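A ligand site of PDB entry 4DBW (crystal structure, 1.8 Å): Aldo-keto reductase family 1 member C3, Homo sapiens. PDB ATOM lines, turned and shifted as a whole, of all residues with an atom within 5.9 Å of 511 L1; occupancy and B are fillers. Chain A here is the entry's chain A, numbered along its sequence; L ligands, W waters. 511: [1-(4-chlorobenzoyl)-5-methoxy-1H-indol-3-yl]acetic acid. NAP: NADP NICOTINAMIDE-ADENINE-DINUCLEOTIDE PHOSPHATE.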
ATOM      1  N   TYR A  24       1.238   8.625   6.835  1.00  0.00           N
ATOM      2  CA  TYR A  24       1.907   9.915   6.773  1.00  0.00           C
ATOM      3  C   TYR A  24       3.246   9.932   7.512  1.00  0.00           C
ATOM      4  O   TYR A  24       3.353   9.476   8.639  1.00  0.00           O
ATOM      5  CB  TYR A  24       1.050  11.096   7.246  1.00  0.00           C
ATOM      6  CG  TYR A  24       1.813  12.378   7.060  1.00  0.00           C
ATOM      7  CD1 TYR A  24       1.934  12.950   5.803  1.00  0.00           C
ATOM      8  CD2 TYR A  24       2.479  12.980   8.129  1.00  0.00           C
ATOM      9  CE1 TYR A  24       2.667  14.104   5.609  1.00  0.00           C
ATOM     10  CE2 TYR A  24       3.213  14.144   7.944  1.00  0.00           C
ATOM     11  CZ  TYR A  24       3.300  14.695   6.667  1.00  0.00           C
ATOM     12  OH  TYR A  24       4.026  15.843   6.450  1.00  0.00           O
ATOM     13  N   ALA A  52      -3.281   9.736   1.282  1.00  0.00           N
ATOM     14  CA  ALA A  52      -3.893  10.998   0.882  1.00  0.00           C
ATOM     15  C   ALA A  52      -3.025  11.683  -0.172  1.00  0.00           C
ATOM     16  O   ALA A  52      -1.817  11.453  -0.226  1.00  0.00           O
ATOM     17  CB  ALA A  52      -4.062  11.912   2.096  1.00  0.00           C
ATOM     18  N   LEU A  54      -2.286  14.652  -0.080  1.00  0.00           N
ATOM     19  CA  LEU A  54      -1.457  15.521   0.747  1.00  0.00           C
ATOM     20  C   LEU A  54      -0.121  14.902   1.166  1.00  0.00           C
ATOM     21  O   LEU A  54       0.858  15.605   1.397  1.00  0.00           O
ATOM     22  CB  LEU A  54      -2.239  15.928   1.994  1.00  0.00           C
ATOM     23  CG  LEU A  54      -1.538  16.839   3.003  1.00  0.00           C
ATOM     24  CD1 LEU A  54      -1.310  18.211   2.393  1.00  0.00           C
ATOM     25  CD2 LEU A  54      -2.350  16.959   4.307  1.00  0.00           C
ATOM     26  N   TYR A  55      -0.086  13.570   1.281  1.00  0.00           N
ATOM     27  CA  TYR A  55       1.033  12.915   1.948  1.00  0.00           C
ATOM     28  C   TYR A  55       2.259  12.710   1.061  1.00  0.00           C
ATOM     29  O   TYR A  55       3.304  12.259   1.535  1.00  0.00           O
ATOM     30  CB  TYR A  55       0.601  11.551   2.528  1.00  0.00           C
ATOM     31  CG  TYR A  55      -0.528  11.618   3.539  1.00  0.00           C
ATOM     32  CD1 TYR A  55      -1.181  10.457   3.932  1.00  0.00           C
ATOM     33  CD2 TYR A  55      -0.944  12.818   4.089  1.00  0.00           C
ATOM     34  CE1 TYR A  55      -2.201  10.488   4.852  1.00  0.00           C
ATOM     35  CE2 TYR A  55      -1.969  12.864   5.015  1.00  0.00           C
ATOM     36  CZ  TYR A  55      -2.597  11.700   5.385  1.00  0.00           C
ATOM     37  OH  TYR A  55      -3.630  11.714   6.303  1.00  0.00           O
ATOM     38  N   LYS A  84      -7.577  10.776   0.012  1.00  0.00           N
ATOM     39  CA  LYS A  84      -8.315  11.945   0.459  1.00  0.00           C
ATOM     40  C   LYS A  84      -8.150  13.098  -0.504  1.00  0.00           C
ATOM     41  O   LYS A  84      -7.068  13.335  -1.048  1.00  0.00           O
ATOM     42  CB  LYS A  84      -7.851  12.363   1.858  1.00  0.00           C
ATOM     43  CG  LYS A  84      -7.810  11.246   2.887  1.00  0.00           C
ATOM     44  CD  LYS A  84      -7.557  11.802   4.282  1.00  0.00           C
ATOM     45  CE  LYS A  84      -7.261  10.717   5.309  1.00  0.00           C
ATOM     46  NZ  LYS A  84      -5.877  10.186   5.157  1.00  0.00           N
ATOM     47  N   TRP A  86      -7.619  16.760  -1.246  1.00  0.00           N
ATOM     48  CA  TRP A  86      -7.023  17.887  -0.555  1.00  0.00           C
ATOM     49  C   TRP A  86      -7.871  19.156  -0.735  1.00  0.00           C
ATOM     50  O   TRP A  86      -8.692  19.254  -1.660  1.00  0.00           O
ATOM     51  CB  TRP A  86      -5.556  18.114  -0.940  1.00  0.00           C
ATOM     52  CG  TRP A  86      -4.970  19.253  -0.169  1.00  0.00           C
ATOM     53  CD1 TRP A  86      -4.406  20.394  -0.682  1.00  0.00           C
ATOM     54  CD2 TRP A  86      -4.951  19.405   1.248  1.00  0.00           C
ATOM     55  NE1 TRP A  86      -4.030  21.225   0.332  1.00  0.00           N
ATOM     56  CE2 TRP A  86      -4.343  20.642   1.535  1.00  0.00           C
ATOM     57  CE3 TRP A  86      -5.378  18.594   2.319  1.00  0.00           C
ATOM     58  CZ2 TRP A  86      -4.157  21.094   2.847  1.00  0.00           C
ATOM     59  CZ3 TRP A  86      -5.186  19.056   3.610  1.00  0.00           C
ATOM     60  CH2 TRP A  86      -4.587  20.291   3.861  1.00  0.00           C
ATOM     61  N   HIS A 117     -10.624  15.630   2.933  1.00  0.00           N
ATOM     62  CA  HIS A 117      -9.565  15.616   3.960  1.00  0.00           C
ATOM     63  C   HIS A 117      -9.890  16.585   5.078  1.00  0.00           C
ATOM     64  O   HIS A 117      -9.575  16.332   6.237  1.00  0.00           O
ATOM     65  CB  HIS A 117      -8.217  15.999   3.341  1.00  0.00           C
ATOM     66  CG  HIS A 117      -7.037  15.512   4.120  1.00  0.00           C
ATOM     67  ND1 HIS A 117      -5.905  15.009   3.508  1.00  0.00           N
ATOM     68  CD2 HIS A 117      -6.800  15.455   5.448  1.00  0.00           C
ATOM     69  CE1 HIS A 117      -5.026  14.664   4.421  1.00  0.00           C
ATOM     70  NE2 HIS A 117      -5.541  14.923   5.608  1.00  0.00           N
ATOM     71  N   SER A 118     -10.509  17.709   4.714  1.00  0.00           N
ATOM     72  CA  SER A 118     -10.757  18.775   5.668  1.00  0.00           C
ATOM     73  C   SER A 118     -11.837  19.714   5.144  1.00  0.00           C
ATOM     74  O   SER A 118     -11.938  19.933   3.936  1.00  0.00           O
ATOM     75  CB  SER A 118      -9.460  19.545   5.937  1.00  0.00           C
ATOM     76  OG  SER A 118      -9.689  20.766   6.612  1.00  0.00           O
ATOM     77  N   PRO A 119     -12.664  20.256   6.047  1.00  0.00           N
ATOM     78  CA  PRO A 119     -13.700  21.184   5.555  1.00  0.00           C
ATOM     79  C   PRO A 119     -13.150  22.578   5.258  1.00  0.00           C
ATOM     80  O   PRO A 119     -13.874  23.409   4.726  1.00  0.00           O
ATOM     81  CB  PRO A 119     -14.682  21.247   6.725  1.00  0.00           C
ATOM     82  CG  PRO A 119     -13.841  20.963   7.939  1.00  0.00           C
ATOM     83  CD  PRO A 119     -12.782  19.991   7.494  1.00  0.00           C
ATOM     84  N   MET A 120     -11.885  22.822   5.590  1.00  0.00           N
ATOM     85  CA  MET A 120     -11.318  24.163   5.432  1.00  0.00           C
ATOM     86  C   MET A 120     -10.734  24.393   4.040  1.00  0.00           C
ATOM     87  O   MET A 120      -9.541  24.207   3.805  1.00  0.00           O
ATOM     88  CB  MET A 120     -10.291  24.433   6.531  1.00  0.00           C
ATOM     89  CG  MET A 120     -10.902  24.376   7.921  1.00  0.00           C
ATOM     90  SD  MET A 120      -9.725  24.528   9.280  1.00  0.00           S
ATOM     91  CE  MET A 120      -8.793  23.007   9.074  1.00  0.00           C
ATOM     92  N   ASN A 167     -12.327  15.350   9.576  1.00  0.00           N
ATOM     93  CA  ASN A 167     -12.213  16.603  10.319  1.00  0.00           C
ATOM     94  C   ASN A 167     -13.459  17.468  10.270  1.00  0.00           C
ATOM     95  O   ASN A 167     -13.377  18.686  10.381  1.00  0.00           O
ATOM     96  CB  ASN A 167     -10.997  17.399   9.857  1.00  0.00           C
ATOM     97  CG  ASN A 167      -9.692  16.669  10.121  1.00  0.00           C
ATOM     98  OD1 ASN A 167      -9.388  16.301  11.255  1.00  0.00           O
ATOM     99  ND2 ASN A 167      -8.912  16.445   9.067  1.00  0.00           N
ATOM    100  N   GLN A 190     -13.368  10.744   9.668  1.00  0.00           N
ATOM    101  CA  GLN A 190     -12.053  10.507  10.230  1.00  0.00           C
ATOM    102  C   GLN A 190     -11.598  11.764  10.957  1.00  0.00           C
ATOM    103  O   GLN A 190     -11.407  12.822  10.353  1.00  0.00           O
ATOM    104  CB  GLN A 190     -11.036  10.116   9.142  1.00  0.00           C
ATOM    105  CG  GLN A 190      -9.631   9.837   9.683  1.00  0.00           C
ATOM    106  CD  GLN A 190      -8.621   9.503   8.591  1.00  0.00           C
ATOM    107  OE1 GLN A 190      -7.532  10.089   8.538  1.00  0.00           O
ATOM    108  NE2 GLN A 190      -8.959   8.563   7.725  1.00  0.00           N
ATOM    109  N   TYR A 216      -7.755   9.188  14.218  1.00  0.00           N
ATOM    110  CA  TYR A 216      -6.356   9.446  13.920  1.00  0.00           C
ATOM    111  C   TYR A 216      -5.641  10.113  15.095  1.00  0.00           C
ATOM    112  O   TYR A 216      -6.270  10.641  16.005  1.00  0.00           O
ATOM    113  CB  TYR A 216      -6.166  10.237  12.614  1.00  0.00           C
ATOM    114  CG  TYR A 216      -6.476  11.715  12.643  1.00  0.00           C
ATOM    115  CD1 TYR A 216      -7.507  12.250  11.871  1.00  0.00           C
ATOM    116  CD2 TYR A 216      -5.727  12.602  13.412  1.00  0.00           C
ATOM    117  CE1 TYR A 216      -7.779  13.589  11.856  1.00  0.00           C
ATOM    118  CE2 TYR A 216      -5.998  13.965  13.404  1.00  0.00           C
ATOM    119  CZ  TYR A 216      -7.024  14.446  12.623  1.00  0.00           C
ATOM    120  OH  TYR A 216      -7.309  15.784  12.603  1.00  0.00           O
ATOM    121  N   ARG A 226       5.414  21.463  13.389  1.00  0.00           N
ATOM    122  CA  ARG A 226       4.596  22.380  12.603  1.00  0.00           C
ATOM    123  C   ARG A 226       3.217  22.656  13.216  1.00  0.00           C
ATOM    124  O   ARG A 226       2.607  23.678  12.910  1.00  0.00           O
ATOM    125  CB  ARG A 226       4.450  21.872  11.165  1.00  0.00           C
ATOM    126  CG  ARG A 226       5.735  21.943  10.354  1.00  0.00           C
ATOM    127  CD  ARG A 226       5.585  21.223   9.035  1.00  0.00           C
ATOM    128  NE  ARG A 226       5.614  19.777   9.193  1.00  0.00           N
ATOM    129  CZ  ARG A 226       5.427  18.911   8.197  1.00  0.00           C
ATOM    130  NH1 ARG A 226       5.472  17.598   8.421  1.00  0.00           N
ATOM    131  NH2 ARG A 226       5.183  19.357   6.972  1.00  0.00           N
ATOM    132  N   TRP A 227       2.733  21.771  14.082  1.00  0.00           N
ATOM    133  CA  TRP A 227       1.384  21.944  14.619  1.00  0.00           C
ATOM    134  C   TRP A 227       1.166  21.441  16.042  1.00  0.00           C
ATOM    135  O   TRP A 227       0.082  21.635  16.594  1.00  0.00           O
ATOM    136  CB  TRP A 227       0.338  21.330  13.673  1.00  0.00           C
ATOM    137  CG  TRP A 227       0.739  20.018  13.086  1.00  0.00           C
ATOM    138  CD1 TRP A 227       0.773  18.809  13.724  1.00  0.00           C
ATOM    139  CD2 TRP A 227       1.167  19.781  11.737  1.00  0.00           C
ATOM    140  NE1 TRP A 227       1.203  17.834  12.858  1.00  0.00           N
ATOM    141  CE2 TRP A 227       1.445  18.399  11.630  1.00  0.00           C
ATOM    142  CE3 TRP A 227       1.342  20.590  10.607  1.00  0.00           C
ATOM    143  CZ2 TRP A 227       1.894  17.810  10.451  1.00  0.00           C
ATOM    144  CZ3 TRP A 227       1.780  20.009   9.432  1.00  0.00           C
ATOM    145  CH2 TRP A 227       2.056  18.637   9.368  1.00  0.00           C
ATOM    146  N   PHE A 306      -3.134  18.636  16.875  1.00  0.00           N
ATOM    147  CA  PHE A 306      -3.030  19.469  15.679  1.00  0.00           C
ATOM    148  C   PHE A 306      -3.564  20.861  15.997  1.00  0.00           C
ATOM    149  O   PHE A 306      -4.757  21.031  16.258  1.00  0.00           O
ATOM    150  CB  PHE A 306      -3.799  18.856  14.504  1.00  0.00           C
ATOM    151  CG  PHE A 306      -3.065  17.728  13.827  1.00  0.00           C
ATOM    152  CD1 PHE A 306      -3.078  16.451  14.373  1.00  0.00           C
ATOM    153  CD2 PHE A 306      -2.374  17.942  12.646  1.00  0.00           C
ATOM    154  CE1 PHE A 306      -2.401  15.412  13.753  1.00  0.00           C
ATOM    155  CE2 PHE A 306      -1.698  16.903  12.026  1.00  0.00           C
ATOM    156  CZ  PHE A 306      -1.715  15.641  12.577  1.00  0.00           C
ATOM    157  N   TYR A 317     -13.423  26.105  10.308  1.00  0.00           N
ATOM    158  CA  TYR A 317     -12.656  25.512  11.402  1.00  0.00           C
ATOM    159  C   TYR A 317     -13.575  24.635  12.244  1.00  0.00           C
ATOM    160  O   TYR A 317     -14.607  25.101  12.728  1.00  0.00           O
ATOM    161  CB  TYR A 317     -12.033  26.626  12.249  1.00  0.00           C
ATOM    162  CG  TYR A 317     -11.125  26.150  13.365  1.00  0.00           C
ATOM    163  CD1 TYR A 317      -9.986  25.389  13.085  1.00  0.00           C
ATOM    164  CD2 TYR A 317     -11.382  26.486  14.686  1.00  0.00           C
ATOM    165  CE1 TYR A 317      -9.150  24.966  14.106  1.00  0.00           C
ATOM    166  CE2 TYR A 317     -10.540  26.070  15.708  1.00  0.00           C
ATOM    167  CZ  TYR A 317      -9.434  25.312  15.414  1.00  0.00           C
ATOM    168  OH  TYR A 317      -8.596  24.900  16.423  1.00  0.00           O
ATOM    169  N   PRO A 318     -13.217  23.352  12.413  1.00  0.00           N
ATOM    170  CA  PRO A 318     -14.124  22.389  13.036  1.00  0.00           C
ATOM    171  C   PRO A 318     -14.229  22.498  14.553  1.00  0.00           C
ATOM    172  O   PRO A 318     -15.208  22.003  15.115  1.00  0.00           O
ATOM    173  CB  PRO A 318     -13.514  21.035  12.641  1.00  0.00           C
ATOM    174  CG  PRO A 318     -12.079  21.318  12.441  1.00  0.00           C
ATOM    175  CD  PRO A 318     -12.010  22.708  11.862  1.00  0.00           C
ATOM    176  N   TYR A 319     -13.261  23.126  15.212  1.00  0.00           N
ATOM    177  CA  TYR A 319     -13.199  23.088  16.674  1.00  0.00           C
ATOM    178  C   TYR A 319     -13.808  24.322  17.358  1.00  0.00           C
ATOM    179  O   TYR A 319     -13.655  24.493  18.572  1.00  0.00           O
ATOM    180  CB  TYR A 319     -11.765  22.880  17.169  1.00  0.00           C
ATOM    181  CG  TYR A 319     -11.146  21.577  16.712  1.00  0.00           C
ATOM    182  CD1 TYR A 319     -11.893  20.404  16.707  1.00  0.00           C
ATOM    183  CD2 TYR A 319      -9.819  21.521  16.307  1.00  0.00           C
ATOM    184  CE1 TYR A 319     -11.319  19.195  16.290  1.00  0.00           C
ATOM    185  CE2 TYR A 319      -9.250  20.327  15.896  1.00  0.00           C
ATOM    186  CZ  TYR A 319     -10.004  19.174  15.883  1.00  0.00           C
ATOM    187  OH  TYR A 319      -9.425  17.984  15.486  1.00  0.00           O
HETATM  188 CL1  511 L   1      -8.882  19.624  12.333  1.00  0.00          CL
HETATM  189  N01 511 L   1      -3.526  18.261   8.110  1.00  0.00           N
HETATM  190  C02 511 L   1      -3.487  16.989   8.697  1.00  0.00           C
HETATM  191  O01 511 L   1      -1.874  12.730   8.445  1.00  0.00           O
HETATM  192  C03 511 L   1      -2.293  16.386   8.450  1.00  0.00           C
HETATM  193  O02 511 L   1      -3.441  13.958   7.432  1.00  0.00           O
HETATM  194  C04 511 L   1      -0.223  17.172   7.139  1.00  0.00           C
HETATM  195  O03 511 L   1       1.589  18.147   5.806  1.00  0.00           O
HETATM  196  C05 511 L   1       0.337  18.200   6.396  1.00  0.00           C
HETATM  197  O04 511 L   1      -4.684  20.003   7.278  1.00  0.00           O
HETATM  198  C06 511 L   1      -0.459  19.368   6.203  1.00  0.00           C
HETATM  199  C07 511 L   1      -1.732  19.510   6.712  1.00  0.00           C
HETATM  200  C08 511 L   1      -1.522  17.295   7.663  1.00  0.00           C
HETATM  201  C09 511 L   1      -2.284  18.448   7.466  1.00  0.00           C
HETATM  202  C10 511 L   1      -1.837  15.034   8.916  1.00  0.00           C
HETATM  203  C11 511 L   1      -2.457  13.898   8.130  1.00  0.00           C
HETATM  204  C12 511 L   1       2.051  19.272   5.101  1.00  0.00           C
HETATM  205  C13 511 L   1      -4.606  19.152   8.157  1.00  0.00           C
HETATM  206  C14 511 L   1      -5.670  19.191   9.189  1.00  0.00           C
HETATM  207  C15 511 L   1      -6.938  19.687   8.845  1.00  0.00           C
HETATM  208  C16 511 L   1      -7.936  19.809   9.810  1.00  0.00           C
HETATM  209  C17 511 L   1      -7.663  19.432  11.132  1.00  0.00           C
HETATM  210  C18 511 L   1      -6.409  18.946  11.489  1.00  0.00           C
HETATM  211  C19 511 L   1      -5.408  18.836  10.512  1.00  0.00           C
HETATM  212  PA  NAP L   2      -0.191   8.059  15.374  1.00  0.00           P
HETATM  213  O1A NAP L   2      -0.858   8.772  16.494  1.00  0.00           O
HETATM  214  O2A NAP L   2      -1.079   6.850  14.824  1.00  0.00           O
HETATM  215  O5B NAP L   2       1.180   7.391  15.883  1.00  0.00           O
HETATM  216  C5B NAP L   2       2.056   8.412  16.379  1.00  0.00           C
HETATM  217  C4B NAP L   2       3.433   7.776  16.653  1.00  0.00           C
HETATM  218  O4B NAP L   2       3.253   6.580  17.410  1.00  0.00           O
HETATM  219  C3B NAP L   2       4.126   7.329  15.357  1.00  0.00           C
HETATM  220  O3B NAP L   2       4.991   8.360  14.879  1.00  0.00           O
HETATM  221  C2B NAP L   2       4.926   6.047  15.772  1.00  0.00           C
HETATM  222  O2B NAP L   2       6.336   6.292  15.756  1.00  0.00           O
HETATM  223  C1B NAP L   2       4.440   5.773  17.225  1.00  0.00           C
HETATM  224  N9A NAP L   2       4.051   4.388  17.453  1.00  0.00           N
HETATM  225  C8A NAP L   2       3.348   3.588  16.608  1.00  0.00           C
HETATM  226  N7A NAP L   2       3.153   2.425  17.165  1.00  0.00           N
HETATM  227  C5A NAP L   2       3.716   2.418  18.396  1.00  0.00           C
HETATM  228  C6A NAP L   2       3.827   1.474  19.428  1.00  0.00           C
HETATM  229  N6A NAP L   2       3.275   0.217  19.288  1.00  0.00           N
HETATM  230  N1A NAP L   2       4.474   1.821  20.532  1.00  0.00           N
HETATM  231  C2A NAP L   2       5.005   3.019  20.675  1.00  0.00           C
HETATM  232  N3A NAP L   2       4.922   3.943  19.736  1.00  0.00           N
HETATM  233  C4A NAP L   2       4.296   3.684  18.600  1.00  0.00           C
HETATM  234  O3  NAP L   2       0.298   9.061  14.200  1.00  0.00           O
HETATM  235  PN  NAP L   2      -0.722   9.991  13.339  1.00  0.00           P
HETATM  236  O1N NAP L   2       0.086  10.276  12.059  1.00  0.00           O
HETATM  237  O2N NAP L   2      -0.985  11.337  14.031  1.00  0.00           O
HETATM  238  O5D NAP L   2      -2.126   9.273  12.983  1.00  0.00           O
HETATM  239  C5D NAP L   2      -1.880   8.102  12.205  1.00  0.00           C
HETATM  240  C4D NAP L   2      -2.425   8.244  10.767  1.00  0.00           C
HETATM  241  O4D NAP L   2      -3.756   8.842  10.750  1.00  0.00           O
HETATM  242  C3D NAP L   2      -1.569   9.195   9.917  1.00  0.00           C
HETATM  243  O3D NAP L   2      -0.390   8.550   9.464  1.00  0.00           O
HETATM  244  C2D NAP L   2      -2.558   9.471   8.776  1.00  0.00           C
HETATM  245  O2D NAP L   2      -2.597   8.341   7.884  1.00  0.00           O
HETATM  246  C1D NAP L   2      -3.904   9.617   9.540  1.00  0.00           C
HETATM  247  N1N NAP L   2      -4.143  11.034   9.874  1.00  0.00           N
HETATM  248  C2N NAP L   2      -5.090  11.704   9.251  1.00  0.00           C
HETATM  249  C3N NAP L   2      -5.330  13.048   9.557  1.00  0.00           C
HETATM  250  C7N NAP L   2      -6.412  13.789   8.875  1.00  0.00           C
HETATM  251  O7N NAP L   2      -6.401  15.011   8.868  1.00  0.00           O
HETATM  252  N7N NAP L   2      -7.400  13.112   8.229  1.00  0.00           N
HETATM  253  C4N NAP L   2      -4.547  13.671  10.526  1.00  0.00           C
HETATM  254  C5N NAP L   2      -3.574  12.930  11.152  1.00  0.00           C
HETATM  255  C6N NAP L   2      -3.398  11.602  10.807  1.00  0.00           C
HETATM  256  P2B NAP L   2       7.147   5.246  14.819  1.00  0.00           P
HETATM  257  O1X NAP L   2       6.908   5.506  13.392  1.00  0.00           O
HETATM  258  O2X NAP L   2       8.695   5.482  15.190  1.00  0.00           O
HETATM  259  O3X NAP L   2       6.699   3.750  15.211  1.00  0.00           O
HETATM  260 CL1  511 L   3      -5.082  22.182  13.040  1.00  0.00          CL
HETATM  261  N01 511 L   3      -1.271  23.131   7.335  1.00  0.00           N
HETATM  262  C02 511 L   3      -0.229  23.435   8.235  1.00  0.00           C
HETATM  263  O01 511 L   3       3.693  25.574   8.771  1.00  0.00           O
HETATM  264  C03 511 L   3       0.985  23.379   7.586  1.00  0.00           C
HETATM  265  O02 511 L   3       1.901  25.829   7.461  1.00  0.00           O
HETATM  266  C04 511 L   3       1.571  22.847   5.120  1.00  0.00           C
HETATM  267  O03 511 L   3       1.815  22.290   2.741  1.00  0.00           O
HETATM  268  C05 511 L   3       1.060  22.512   3.872  1.00  0.00           C
HETATM  269  O04 511 L   3      -3.425  23.336   6.725  1.00  0.00           O
HETATM  270  C06 511 L   3      -0.351  22.370   3.767  1.00  0.00           C
HETATM  271  C07 511 L   3      -1.219  22.546   4.829  1.00  0.00           C
HETATM  272  C08 511 L   3       0.708  23.041   6.224  1.00  0.00           C
HETATM  273  C09 511 L   3      -0.676  22.893   6.088  1.00  0.00           C
HETATM  274  C10 511 L   3       2.330  23.621   8.192  1.00  0.00           C
HETATM  275  C11 511 L   3       2.726  25.087   8.215  1.00  0.00           C
HETATM  276  C12 511 L   3       3.222  22.360   2.848  1.00  0.00           C
HETATM  277  C13 511 L   3      -2.629  23.132   7.640  1.00  0.00           C
HETATM  278  C14 511 L   3      -3.203  22.897   9.006  1.00  0.00           C
HETATM  279  C15 511 L   3      -2.509  22.145   9.972  1.00  0.00           C
HETATM  280  C16 511 L   3      -3.097  21.922  11.208  1.00  0.00           C
HETATM  281  C17 511 L   3      -4.363  22.450  11.496  1.00  0.00           C
HETATM  282  C18 511 L   3      -5.050  23.196  10.534  1.00  0.00           C
HETATM  283  C19 511 L   3      -4.468  23.411   9.297  1.00  0.00           C
HETATM  284  O   HOH W   1      -5.925  22.310   6.614  1.00  0.00           O
HETATM  285  O   HOH W   2       0.004  12.603  10.554  1.00  0.00           O
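A ring nitrogen (NE2) of His 117 sits at hydrogen-bond distance from an oxygen (O02) of 511 L1, 2.9 Å away. The side-chain amide nitrogen (ND2) of Asn 167 is in hydrogen-bond range of an oxygen (O7N) of NAP L2, at 2.9 Å. OH of Tyr 24 sits at hydrogen-bond distance from O03 of 511 L1 (3.4 Å). The backbone NH (N) of Tyr 24 lies within hydrogen-bond range of an oxygen (O3D) of NAP L2. A ring nitrogen (NE2) of His 117 lies within hydrogen-bond range of an oxygen (O7N) of NAP L2 (3.4 Å). OH of Tyr 55 sits at hydrogen-bond distance from O02 of 511 L1, 2.5 Å away. The side-chain amide oxygen of Gln 190 sits close to a nitrogen (N7N) of NAP L2 (3.0 Å).
OH of Tyr 216 lies within hydrogen-bond range of OD1 of Asn 167, at 2.5 Å. O of His 117 is in hydrogen-bond range of ND2 of Asn 167, at 2.9 Å. The backbone NH (N) of Asn 167 lies within hydrogen-bond range of the backbone carbonyl oxygen (O) of Gln 190 (2.8 Å). The backbone NH of Met 120 lies close to the side-chain hydroxyl of Ser 118 (3.2 Å). The side-chain hydroxyl (OH) of Tyr 24 sits at hydrogen-bond distance from the guanidinium group (NH1) of Arg 226, 3.0 Å away. The side-chain amino group (NZ) of Lys 84 is in hydrogen-bond range of the side-chain hydroxyl (OH) of Tyr 55, at 2.9 Å.
Merely in contact with 511 L1: Leu 54, Trp 86, Ser 118, Met 120, Asn 167, Tyr 216, Arg 226, Trp 227, Phe 306, Pro 318 and Tyr 319. Hydrophobic or aromatic side chains within 4 Å of 511 L1: Tyr 24, Leu 54, Tyr 55, Trp 86, His 117, Met 120, Trp 227, Phe 306, Pro 318 and Tyr 319. Within 4 Å of 511 L1: Tyr 24, Leu 54, Tyr 55, Trp 86, His 117, Ser 118, Met 120, Asn 167, Tyr 216, Arg 226, Trp 227, Phe 306, Pro 318 and Tyr 319. The nearest printed residue that does not touch 511 L1 is Lys 84 (5.0 Å).
Water W1 bridges O04 of 511 L1 (2.7 Å) and O04 of 511 L3 (2.7 Å). Water W2 lies within hydrogen-bond range of an oxygen (O1N) of NAP L2 (2.8 Å) and an oxygen (O01) of 511 L1 (2.8 Å).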
